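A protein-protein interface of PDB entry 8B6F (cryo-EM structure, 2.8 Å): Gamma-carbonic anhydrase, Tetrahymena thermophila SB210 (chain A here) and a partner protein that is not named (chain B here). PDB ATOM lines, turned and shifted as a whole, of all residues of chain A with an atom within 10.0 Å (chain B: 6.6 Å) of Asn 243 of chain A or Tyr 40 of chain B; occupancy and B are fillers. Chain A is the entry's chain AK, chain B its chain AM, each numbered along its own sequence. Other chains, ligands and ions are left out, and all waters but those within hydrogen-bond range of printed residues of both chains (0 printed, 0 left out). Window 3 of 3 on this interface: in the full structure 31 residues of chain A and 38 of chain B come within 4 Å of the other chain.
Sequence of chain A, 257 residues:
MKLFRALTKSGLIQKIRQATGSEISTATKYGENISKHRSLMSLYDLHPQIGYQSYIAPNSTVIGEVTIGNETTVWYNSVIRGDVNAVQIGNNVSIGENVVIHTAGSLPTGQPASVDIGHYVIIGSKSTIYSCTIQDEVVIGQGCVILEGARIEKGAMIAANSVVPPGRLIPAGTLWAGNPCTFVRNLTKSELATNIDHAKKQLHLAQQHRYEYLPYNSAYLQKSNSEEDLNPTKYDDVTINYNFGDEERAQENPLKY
CD1 of Tyr 216 of chain A touches CD of Arg 28 of chain B, 3.6 Å away. Tyr 220 of chain A touches Ser 38 of chain B (CB to O, 3.3 Å). CA of Cys 39 of chain B touches CE2 of Tyr 220 of chain A (3.7 Å). Tyr 220 of chain A touches Leu 43 of chain B. Leu 43 of chain B touches Lys 223 of chain A. OH of Tyr 242 of chain A touches O of Tyr 40 of chain B (3.7 Å). Tyr 40 of chain B touches Asn 243 of chain A. Pro 42 of chain B touches Tyr 257 of chain A.
Hydrophobic or aromatic side chains of chain B that line the printed part of chain A: Tyr 40, Pro 42 and Leu 43. Among the printed residues, 10 pairs touch across the chains. Among the printed residues, Asp or Glu carboxylates within 4 Å of a Lys or Arg side-chain nitrogen of the other chain: Lys 223 of chain A with Glu 41 of chain B.
NZ of Lys 223 of chain A is in salt-bridge range of OE2 of Glu 41 of chain B, at 2.9 Å. ND2 of Asn 217 of chain A lies within hydrogen-bond range of O of Leu 43 of chain B (3.2 Å).
Of the printed residues of chain B, Tyr 216 of chain A touches Arg 28 (3.6 Å). Asn 243 of chain A touches just one residue of chain B: Tyr 40. Of the printed residues of chain A, Arg 28 of chain B touches Tyr 216. No residue of chain A comes within 4 Å of Lys 32 of chain B. No residue of chain A comes within 4 Å of Ile 37 of chain B. Ser 38 of chain B touches just one residue of chain A: Tyr 220 (3.3 Å). Of the printed residues of chain A, Glu 41 of chain B touches Lys 223 (2.9 Å). Printed residues of chain A within 4 Å of Leu 43 of chain B: Asn 217 (3.2 Å), Tyr 220 (3.9 Å) and Lys 223 (3.8 Å). The nearest residue of chain B that does not touch Asn 243 of chain A is Lys 32 of chain B (4.4 Å). The nearest printed residue of chain B that does not touch Lys 223 of chain A is Ser 38 of chain B (7.3 Å).
The side-chain carboxylate (OD1) of Asp 36 of chain B sits at hydrogen-bond distance from the backbone NH (N) of Ser 38 of chain B (2.6 Å). The side-chain amide oxygen (OD1) of Asn 217 of chain A is in hydrogen-bond range of the backbone NH (N) of Ala 219 of chain A (2.7 Å). SG of Cys 31 of chain B lies within hydrogen-bond range of OG of Ser 38 of chain B (3.6 Å).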
ATOM      1  N   ARG A  38      20.902   3.998  -5.271  1.00  0.00           N
ATOM      2  CA  ARG A  38      20.249   5.156  -4.678  1.00  0.00           C
ATOM      3  C   ARG A  38      18.943   5.424  -5.409  1.00  0.00           C
ATOM      4  O   ARG A  38      18.888   5.359  -6.640  1.00  0.00           O
ATOM      5  CB  ARG A  38      21.143   6.395  -4.746  1.00  0.00           C
ATOM      6  CG  ARG A  38      22.416   6.284  -3.926  1.00  0.00           C
ATOM      7  CD  ARG A  38      23.365   7.417  -4.254  1.00  0.00           C
ATOM      8  NE  ARG A  38      23.835   7.335  -5.631  1.00  0.00           N
ATOM      9  CZ  ARG A  38      24.466   8.311  -6.267  1.00  0.00           C
ATOM     10  NH1 ARG A  38      24.706   9.473  -5.686  1.00  0.00           N
ATOM     11  NH2 ARG A  38      24.864   8.115  -7.520  1.00  0.00           N
ATOM     12  N   PRO A 215      13.508   9.236  10.464  1.00  0.00           N
ATOM     13  CA  PRO A 215      14.222  10.242   9.658  1.00  0.00           C
ATOM     14  C   PRO A 215      15.718  10.005   9.565  1.00  0.00           C
ATOM     15  O   PRO A 215      16.354  10.539   8.649  1.00  0.00           O
ATOM     16  CB  PRO A 215      13.904  11.558  10.380  1.00  0.00           C
ATOM     17  CG  PRO A 215      13.590  11.160  11.772  1.00  0.00           C
ATOM     18  CD  PRO A 215      12.916   9.825  11.677  1.00  0.00           C
ATOM     19  N   TYR A 216      16.301   9.233  10.477  1.00  0.00           N
ATOM     20  CA  TYR A 216      17.735   8.970  10.493  1.00  0.00           C
ATOM     21  C   TYR A 216      17.978   7.541  10.029  1.00  0.00           C
ATOM     22  O   TYR A 216      17.435   6.596  10.609  1.00  0.00           O
ATOM     23  CB  TYR A 216      18.312   9.183  11.892  1.00  0.00           C
ATOM     24  CG  TYR A 216      17.972  10.524  12.497  1.00  0.00           C
ATOM     25  CD1 TYR A 216      18.644  11.674  12.109  1.00  0.00           C
ATOM     26  CD2 TYR A 216      16.983  10.635  13.464  1.00  0.00           C
ATOM     27  CE1 TYR A 216      18.338  12.900  12.664  1.00  0.00           C
ATOM     28  CE2 TYR A 216      16.669  11.855  14.025  1.00  0.00           C
ATOM     29  CZ  TYR A 216      17.348  12.985  13.621  1.00  0.00           C
ATOM     30  OH  TYR A 216      17.038  14.203  14.178  1.00  0.00           O
ATOM     31  N   ASN A 217      18.791   7.388   8.988  1.00  0.00           N
ATOM     32  CA  ASN A 217      19.142   6.068   8.483  1.00  0.00           C
ATOM     33  C   ASN A 217      20.180   5.427   9.397  1.00  0.00           C
ATOM     34  O   ASN A 217      21.168   6.065   9.771  1.00  0.00           O
ATOM     35  CB  ASN A 217      19.680   6.179   7.056  1.00  0.00           C
ATOM     36  CG  ASN A 217      19.904   4.829   6.410  1.00  0.00           C
ATOM     37  OD1 ASN A 217      19.906   3.798   7.079  1.00  0.00           O
ATOM     38  ND2 ASN A 217      20.101   4.831   5.099  1.00  0.00           N
ATOM     39  N   SER A 218      19.953   4.165   9.758  1.00  0.00           N
ATOM     40  CA  SER A 218      20.845   3.431  10.647  1.00  0.00           C
ATOM     41  C   SER A 218      21.671   2.380   9.918  1.00  0.00           C
ATOM     42  O   SER A 218      22.343   1.575  10.568  1.00  0.00           O
ATOM     43  CB  SER A 218      20.041   2.772  11.768  1.00  0.00           C
ATOM     44  OG  SER A 218      19.097   1.855  11.245  1.00  0.00           O
ATOM     45  N   ALA A 219      21.638   2.365   8.585  1.00  0.00           N
ATOM     46  CA  ALA A 219      22.393   1.364   7.840  1.00  0.00           C
ATOM     47  C   ALA A 219      23.893   1.577   7.989  1.00  0.00           C
ATOM     48  O   ALA A 219      24.661   0.610   8.032  1.00  0.00           O
ATOM     49  CB  ALA A 219      21.993   1.393   6.367  1.00  0.00           C
ATOM     50  N   TYR A 220      24.332   2.835   8.067  1.00  0.00           N
ATOM     51  CA  TYR A 220      25.761   3.112   8.164  1.00  0.00           C
ATOM     52  C   TYR A 220      26.365   2.512   9.426  1.00  0.00           C
ATOM     53  O   TYR A 220      27.561   2.206   9.456  1.00  0.00           O
ATOM     54  CB  TYR A 220      26.009   4.620   8.127  1.00  0.00           C
ATOM     55  CG  TYR A 220      25.624   5.335   9.400  1.00  0.00           C
ATOM     56  CD1 TYR A 220      24.311   5.715   9.639  1.00  0.00           C
ATOM     57  CD2 TYR A 220      26.578   5.637  10.361  1.00  0.00           C
ATOM     58  CE1 TYR A 220      23.958   6.370  10.803  1.00  0.00           C
ATOM     59  CE2 TYR A 220      26.236   6.292  11.527  1.00  0.00           C
ATOM     60  CZ  TYR A 220      24.926   6.656  11.741  1.00  0.00           C
ATOM     61  OH  TYR A 220      24.584   7.308  12.902  1.00  0.00           O
ATOM     62  N   LEU A 221      25.562   2.341  10.475  1.00  0.00           N
ATOM     63  CA  LEU A 221      26.058   1.779  11.723  1.00  0.00           C
ATOM     64  C   LEU A 221      26.390   0.297  11.615  1.00  0.00           C
ATOM     65  O   LEU A 221      27.003  -0.249  12.537  1.00  0.00           O
ATOM     66  CB  LEU A 221      25.027   1.989  12.831  1.00  0.00           C
ATOM     67  CG  LEU A 221      24.772   3.439  13.243  1.00  0.00           C
ATOM     68  CD1 LEU A 221      23.580   3.530  14.175  1.00  0.00           C
ATOM     69  CD2 LEU A 221      26.001   4.021  13.904  1.00  0.00           C
ATOM     70  N   LYS A 223      28.114  -1.138   8.990  1.00  0.00           N
ATOM     71  CA  LYS A 223      29.265  -1.373   8.131  1.00  0.00           C
ATOM     72  C   LYS A 223      30.547  -1.437   8.954  1.00  0.00           C
ATOM     73  O   LYS A 223      30.612  -0.972  10.093  1.00  0.00           O
ATOM     74  CB  LYS A 223      29.381  -0.275   7.074  1.00  0.00           C
ATOM     75  CG  LYS A 223      28.264  -0.286   6.046  1.00  0.00           C
ATOM     76  CD  LYS A 223      28.454   0.796   4.994  1.00  0.00           C
ATOM     77  CE  LYS A 223      29.677   0.535   4.129  1.00  0.00           C
ATOM     78  NZ  LYS A 223      29.781   1.514   3.012  1.00  0.00           N
ATOM     79  N   THR A 239      33.555  23.738   1.567  1.00  0.00           N
ATOM     80  CA  THR A 239      32.743  24.757   0.912  1.00  0.00           C
ATOM     81  C   THR A 239      31.401  24.947   1.614  1.00  0.00           C
ATOM     82  O   THR A 239      31.112  26.030   2.127  1.00  0.00           O
ATOM     83  CB  THR A 239      32.520  24.388  -0.561  1.00  0.00           C
ATOM     84  OG1 THR A 239      31.821  23.140  -0.648  1.00  0.00           O
ATOM     85  CG2 THR A 239      33.849  24.277  -1.291  1.00  0.00           C
ATOM     86  N   ILE A 240      30.581  23.903   1.652  1.00  0.00           N
ATOM     87  CA  ILE A 240      29.277  23.970   2.301  1.00  0.00           C
ATOM     88  C   ILE A 240      28.797  22.545   2.528  1.00  0.00           C
ATOM     89  O   ILE A 240      29.024  21.660   1.700  1.00  0.00           O
ATOM     90  CB  ILE A 240      28.272  24.790   1.456  1.00  0.00           C
ATOM     91  CG1 ILE A 240      26.930  24.934   2.181  1.00  0.00           C
ATOM     92  CG2 ILE A 240      28.051  24.137   0.100  1.00  0.00           C
ATOM     93  CD1 ILE A 240      26.997  25.769   3.433  1.00  0.00           C
ATOM     94  N   ASN A 241      28.127  22.332   3.655  1.00  0.00           N
ATOM     95  CA  ASN A 241      27.529  21.042   3.964  1.00  0.00           C
ATOM     96  C   ASN A 241      26.126  21.000   3.380  1.00  0.00           C
ATOM     97  O   ASN A 241      25.329  21.916   3.599  1.00  0.00           O
ATOM     98  CB  ASN A 241      27.482  20.809   5.473  1.00  0.00           C
ATOM     99  CG  ASN A 241      28.851  20.583   6.071  1.00  0.00           C
ATOM    100  OD1 ASN A 241      29.871  20.844   5.435  1.00  0.00           O
ATOM    101  ND2 ASN A 241      28.883  20.099   7.305  1.00  0.00           N
ATOM    102  N   TYR A 242      25.829  19.935   2.635  1.00  0.00           N
ATOM    103  CA  TYR A 242      24.520  19.840   2.001  1.00  0.00           C
ATOM    104  C   TYR A 242      23.399  19.929   3.024  1.00  0.00           C
ATOM    105  O   TYR A 242      22.307  20.413   2.706  1.00  0.00           O
ATOM    106  CB  TYR A 242      24.411  18.542   1.201  1.00  0.00           C
ATOM    107  CG  TYR A 242      24.234  17.310   2.055  1.00  0.00           C
ATOM    108  CD1 TYR A 242      25.315  16.718   2.690  1.00  0.00           C
ATOM    109  CD2 TYR A 242      22.981  16.736   2.219  1.00  0.00           C
ATOM    110  CE1 TYR A 242      25.152  15.593   3.471  1.00  0.00           C
ATOM    111  CE2 TYR A 242      22.809  15.612   2.997  1.00  0.00           C
ATOM    112  CZ  TYR A 242      23.897  15.044   3.619  1.00  0.00           C
ATOM    113  OH  TYR A 242      23.726  13.923   4.393  1.00  0.00           O
ATOM    114  N   ASN A 243      23.644  19.469   4.245  1.00  0.00           N
ATOM    115  CA  ASN A 243      22.659  19.540   5.323  1.00  0.00           C
ATOM    116  C   ASN A 243      22.914  20.768   6.195  1.00  0.00           C
ATOM    117  O   ASN A 243      23.088  20.683   7.409  1.00  0.00           O
ATOM    118  CB  ASN A 243      22.692  18.259   6.148  1.00  0.00           C
ATOM    119  CG  ASN A 243      24.025  18.042   6.827  1.00  0.00           C
ATOM    120  OD1 ASN A 243      25.062  18.494   6.344  1.00  0.00           O
ATOM    121  ND2 ASN A 243      24.006  17.350   7.958  1.00  0.00           N
ATOM    122  N   PHE A 244      22.934  21.931   5.551  1.00  0.00           N
ATOM    123  CA  PHE A 244      23.111  23.198   6.248  1.00  0.00           C
ATOM    124  C   PHE A 244      21.740  23.734   6.639  1.00  0.00           C
ATOM    125  O   PHE A 244      20.865  23.895   5.783  1.00  0.00           O
ATOM    126  CB  PHE A 244      23.856  24.206   5.373  1.00  0.00           C
ATOM    127  CG  PHE A 244      24.195  25.488   6.081  1.00  0.00           C
ATOM    128  CD1 PHE A 244      25.202  25.526   7.030  1.00  0.00           C
ATOM    129  CD2 PHE A 244      23.511  26.658   5.789  1.00  0.00           C
ATOM    130  CE1 PHE A 244      25.517  26.706   7.680  1.00  0.00           C
ATOM    131  CE2 PHE A 244      23.822  27.840   6.436  1.00  0.00           C
ATOM    132  CZ  PHE A 244      24.826  27.864   7.382  1.00  0.00           C
ATOM    133  N   GLY A 245      21.559  24.007   7.926  1.00  0.00           N
ATOM    134  CA  GLY A 245      20.260  24.385   8.434  1.00  0.00           C
ATOM    135  C   GLY A 245      19.308  23.233   8.650  1.00  0.00           C
ATOM    136  O   GLY A 245      18.117  23.473   8.881  1.00  0.00           O
ATOM    137  N   ASP A 246      19.788  21.990   8.580  1.00  0.00           N
ATOM    138  CA  ASP A 246      18.917  20.841   8.795  1.00  0.00           C
ATOM    139  C   ASP A 246      18.532  20.672  10.257  1.00  0.00           C
ATOM    140  O   ASP A 246      17.592  19.929  10.553  1.00  0.00           O
ATOM    141  CB  ASP A 246      19.578  19.564   8.279  1.00  0.00           C
ATOM    142  CG  ASP A 246      19.396  19.382   6.784  1.00  0.00           C
ATOM    143  OD1 ASP A 246      18.947  20.335   6.115  1.00  0.00           O
ATOM    144  OD2 ASP A 246      19.688  18.278   6.278  1.00  0.00           O
ATOM    145  N   GLU A 247      19.234  21.334  11.176  1.00  0.00           N
ATOM    146  CA  GLU A 247      18.779  21.357  12.560  1.00  0.00           C
ATOM    147  C   GLU A 247      17.498  22.166  12.710  1.00  0.00           C
ATOM    148  O   GLU A 247      16.826  22.057  13.739  1.00  0.00           O
ATOM    149  CB  GLU A 247      19.873  21.912  13.479  1.00  0.00           C
ATOM    150  CG  GLU A 247      20.064  23.426  13.448  1.00  0.00           C
ATOM    151  CD  GLU A 247      20.570  23.935  12.115  1.00  0.00           C
ATOM    152  OE1 GLU A 247      20.928  23.101  11.258  1.00  0.00           O
ATOM    153  OE2 GLU A 247      20.612  25.168  11.925  1.00  0.00           O
ATOM    154  N   GLU A 248      17.154  22.975  11.704  1.00  0.00           N
ATOM    155  CA  GLU A 248      15.899  23.708  11.674  1.00  0.00           C
ATOM    156  C   GLU A 248      14.939  23.215  10.603  1.00  0.00           C
ATOM    157  O   GLU A 248      13.741  23.493  10.698  1.00  0.00           O
ATOM    158  CB  GLU A 248      16.167  25.203  11.445  1.00  0.00           C
ATOM    159  CG  GLU A 248      17.105  25.816  12.469  1.00  0.00           C
ATOM    160  CD  GLU A 248      17.470  27.243  12.133  1.00  0.00           C
ATOM    161  OE1 GLU A 248      16.966  27.760  11.115  1.00  0.00           O
ATOM    162  OE2 GLU A 248      18.264  27.848  12.884  1.00  0.00           O
ATOM    163  N   ARG A 249      15.431  22.510   9.589  1.00  0.00           N
ATOM    164  CA  ARG A 249      14.552  21.922   8.589  1.00  0.00           C
ATOM    165  C   ARG A 249      13.737  20.792   9.204  1.00  0.00           C
ATOM    166  O   ARG A 249      14.228  20.040  10.051  1.00  0.00           O
ATOM    167  CB  ARG A 249      15.369  21.402   7.410  1.00  0.00           C
ATOM    168  CG  ARG A 249      14.538  20.783   6.301  1.00  0.00           C
ATOM    169  CD  ARG A 249      15.414  20.372   5.134  1.00  0.00           C
ATOM    170  NE  ARG A 249      14.647  19.738   4.070  1.00  0.00           N
ATOM    171  CZ  ARG A 249      15.159  19.344   2.914  1.00  0.00           C
ATOM    172  NH1 ARG A 249      16.439  19.511   2.632  1.00  0.00           N
ATOM    173  NH2 ARG A 249      14.366  18.770   2.014  1.00  0.00           N
ATOM    174  N   LYS A 256      15.001  10.933   3.250  1.00  0.00           N
ATOM    175  CA  LYS A 256      15.740  12.086   2.755  1.00  0.00           C
ATOM    176  C   LYS A 256      17.196  11.957   3.170  1.00  0.00           C
ATOM    177  O   LYS A 256      17.492  11.676   4.336  1.00  0.00           O
ATOM    178  CB  LYS A 256      15.138  13.389   3.290  1.00  0.00           C
ATOM    179  CG  LYS A 256      15.871  14.648   2.851  1.00  0.00           C
ATOM    180  CD  LYS A 256      16.847  15.125   3.915  1.00  0.00           C
ATOM    181  CE  LYS A 256      17.666  16.305   3.423  1.00  0.00           C
ATOM    182  NZ  LYS A 256      18.665  16.747   4.436  1.00  0.00           N
ATOM    183  N   TYR A 257      18.100  12.158   2.216  1.00  0.00           N
ATOM    184  CA  TYR A 257      19.530  12.062   2.483  1.00  0.00           C
ATOM    185  C   TYR A 257      19.948  13.060   3.556  1.00  0.00           C
ATOM    186  O   TYR A 257      19.892  14.270   3.343  1.00  0.00           O
ATOM    187  CB  TYR A 257      20.335  12.304   1.205  1.00  0.00           C
ATOM    188  CG  TYR A 257      20.036  11.330   0.086  1.00  0.00           C
ATOM    189  CD1 TYR A 257      19.616  10.034   0.354  1.00  0.00           C
ATOM    190  CD2 TYR A 257      20.177  11.709  -1.241  1.00  0.00           C
ATOM    191  CE1 TYR A 257      19.344   9.143  -0.666  1.00  0.00           C
ATOM    192  CE2 TYR A 257      19.906  10.828  -2.270  1.00  0.00           C
ATOM    193  CZ  TYR A 257      19.491   9.547  -1.975  1.00  0.00           C
ATOM    194  OH  TYR A 257      19.222   8.668  -2.995  1.00  0.00           O
ATOM    195  N   ARG B  28      24.269  11.357  15.422  1.00  0.00           N
ATOM    196  CA  ARG B  28      24.568  12.321  14.369  1.00  0.00           C
ATOM    197  C   ARG B  28      25.284  13.542  14.930  1.00  0.00           C
ATOM    198  O   ARG B  28      26.241  14.040  14.328  1.00  0.00           O
ATOM    199  CB  ARG B  28      23.288  12.742  13.651  1.00  0.00           C
ATOM    200  CG  ARG B  28      22.857  11.789  12.554  1.00  0.00           C
ATOM    201  CD  ARG B  28      22.106  12.530  11.461  1.00  0.00           C
ATOM    202  NE  ARG B  28      21.874  11.686  10.296  1.00  0.00           N
ATOM    203  CZ  ARG B  28      21.476  12.134   9.114  1.00  0.00           C
ATOM    204  NH1 ARG B  28      21.253  13.421   8.901  1.00  0.00           N
ATOM    205  NH2 ARG B  28      21.302  11.271   8.117  1.00  0.00           N
ATOM    206  N   CYS B  31      28.838  12.669  15.588  1.00  0.00           N
ATOM    207  CA  CYS B  31      29.585  12.670  14.335  1.00  0.00           C
ATOM    208  C   CYS B  31      29.941  14.089  13.913  1.00  0.00           C
ATOM    209  O   CYS B  31      31.069  14.352  13.483  1.00  0.00           O
ATOM    210  CB  CYS B  31      28.775  11.979  13.239  1.00  0.00           C
ATOM    211  SG  CYS B  31      28.598  10.197  13.445  1.00  0.00           S
ATOM    212  N   LYS B  32      28.991  15.018  14.028  1.00  0.00           N
ATOM    213  CA  LYS B  32      29.261  16.406  13.665  1.00  0.00           C
ATOM    214  C   LYS B  32      30.380  16.982  14.521  1.00  0.00           C
ATOM    215  O   LYS B  32      31.233  17.725  14.025  1.00  0.00           O
ATOM    216  CB  LYS B  32      27.991  17.242  13.805  1.00  0.00           C
ATOM    217  CG  LYS B  32      26.888  16.854  12.834  1.00  0.00           C
ATOM    218  CD  LYS B  32      25.578  17.548  13.174  1.00  0.00           C
ATOM    219  CE  LYS B  32      24.434  17.013  12.326  1.00  0.00           C
ATOM    220  NZ  LYS B  32      23.125  17.603  12.727  1.00  0.00           N
ATOM    221  N   ASP B  36      33.225  13.413  11.674  1.00  0.00           N
ATOM    222  CA  ASP B  36      33.026  12.083  11.111  1.00  0.00           C
ATOM    223  C   ASP B  36      31.874  12.137  10.111  1.00  0.00           C
ATOM    224  O   ASP B  36      30.817  12.696  10.415  1.00  0.00           O
ATOM    225  CB  ASP B  36      32.744  11.085  12.235  1.00  0.00           C
ATOM    226  CG  ASP B  36      32.653   9.662  11.747  1.00  0.00           C
ATOM    227  OD1 ASP B  36      31.930   9.402  10.764  1.00  0.00           O
ATOM    228  OD2 ASP B  36      33.310   8.797  12.358  1.00  0.00           O
ATOM    229  N   ILE B  37      32.077  11.564   8.921  1.00  0.00           N
ATOM    230  CA  ILE B  37      31.092  11.636   7.839  1.00  0.00           C
ATOM    231  C   ILE B  37      30.256  10.358   7.720  1.00  0.00           C
ATOM    232  O   ILE B  37      29.507  10.204   6.753  1.00  0.00           O
ATOM    233  CB  ILE B  37      31.745  12.004   6.496  1.00  0.00           C
ATOM    234  CG1 ILE B  37      32.926  11.093   6.182  1.00  0.00           C
ATOM    235  CG2 ILE B  37      32.176  13.467   6.505  1.00  0.00           C
ATOM    236  CD1 ILE B  37      33.403  11.226   4.755  1.00  0.00           C
ATOM    237  N   SER B  38      30.372   9.437   8.678  1.00  0.00           N
ATOM    238  CA  SER B  38      29.740   8.121   8.566  1.00  0.00           C
ATOM    239  C   SER B  38      28.219   8.233   8.470  1.00  0.00           C
ATOM    240  O   SER B  38      27.583   7.512   7.693  1.00  0.00           O
ATOM    241  CB  SER B  38      30.146   7.243   9.748  1.00  0.00           C
ATOM    242  OG  SER B  38      29.681   7.783  10.970  1.00  0.00           O
ATOM    243  N   CYS B  39      27.624   9.134   9.252  1.00  0.00           N
ATOM    244  CA  CYS B  39      26.171   9.297   9.291  1.00  0.00           C
ATOM    245  C   CYS B  39      25.631   9.742   7.937  1.00  0.00           C
ATOM    246  O   CYS B  39      24.554   9.306   7.515  1.00  0.00           O
ATOM    247  CB  CYS B  39      25.784  10.300  10.378  1.00  0.00           C
ATOM    248  SG  CYS B  39      26.769  11.814  10.388  1.00  0.00           S
ATOM    249  N   TYR B  40      26.366  10.607   7.245  1.00  0.00           N
ATOM    250  CA  TYR B  40      25.921  11.217   5.997  1.00  0.00           C
ATOM    251  C   TYR B  40      25.729  10.204   4.873  1.00  0.00           C
ATOM    252  O   TYR B  40      24.987  10.490   3.930  1.00  0.00           O
ATOM    253  CB  TYR B  40      26.925  12.279   5.552  1.00  0.00           C
ATOM    254  CG  TYR B  40      27.209  13.326   6.601  1.00  0.00           C
ATOM    255  CD1 TYR B  40      26.213  13.764   7.463  1.00  0.00           C
ATOM    256  CD2 TYR B  40      28.478  13.872   6.733  1.00  0.00           C
ATOM    257  CE1 TYR B  40      26.472  14.719   8.425  1.00  0.00           C
ATOM    258  CE2 TYR B  40      28.747  14.828   7.689  1.00  0.00           C
ATOM    259  CZ  TYR B  40      27.741  15.247   8.534  1.00  0.00           C
ATOM    260  OH  TYR B  40      28.010  16.201   9.488  1.00  0.00           O
ATOM    261  N   GLU B  41      26.374   9.045   4.935  1.00  0.00           N
ATOM    262  CA  GLU B  41      26.393   8.144   3.791  1.00  0.00           C
ATOM    263  C   GLU B  41      24.987   7.754   3.357  1.00  0.00           C
ATOM    264  O   GLU B  41      24.149   7.412   4.204  1.00  0.00           O
ATOM    265  CB  GLU B  41      27.140   6.855   4.133  1.00  0.00           C
ATOM    266  CG  GLU B  41      27.324   5.940   2.928  1.00  0.00           C
ATOM    267  CD  GLU B  41      28.367   4.864   3.145  1.00  0.00           C
ATOM    268  OE1 GLU B  41      28.924   4.783   4.260  1.00  0.00           O
ATOM    269  OE2 GLU B  41      28.612   4.081   2.203  1.00  0.00           O
ATOM    270  N   PRO B  42      24.692   7.781   2.049  1.00  0.00           N
ATOM    271  CA  PRO B  42      23.373   7.356   1.579  1.00  0.00           C
ATOM    272  C   PRO B  42      23.425   5.895   1.191  1.00  0.00           C
ATOM    273  O   PRO B  42      24.161   5.502   0.281  1.00  0.00           O
ATOM    274  CB  PRO B  42      23.141   8.259   0.367  1.00  0.00           C
ATOM    275  CG  PRO B  42      24.521   8.417  -0.210  1.00  0.00           C
ATOM    276  CD  PRO B  42      25.513   8.286   0.934  1.00  0.00           C
ATOM    277  N   LEU B  43      22.634   5.089   1.877  1.00  0.00           N
ATOM    278  CA  LEU B  43      22.592   3.658   1.660  1.00  0.00           C
ATOM    279  C   LEU B  43      21.135   3.271   1.500  1.00  0.00           C
ATOM    280  O   LEU B  43      20.249   3.927   2.052  1.00  0.00           O
ATOM    281  CB  LEU B  43      23.228   2.942   2.856  1.00  0.00           C
ATOM    282  CG  LEU B  43      24.757   2.884   2.840  1.00  0.00           C
ATOM    283  CD1 LEU B  43      25.293   2.857   4.262  1.00  0.00           C
ATOM    284  CD2 LEU B  43      25.261   1.678   2.077  1.00  0.00           C
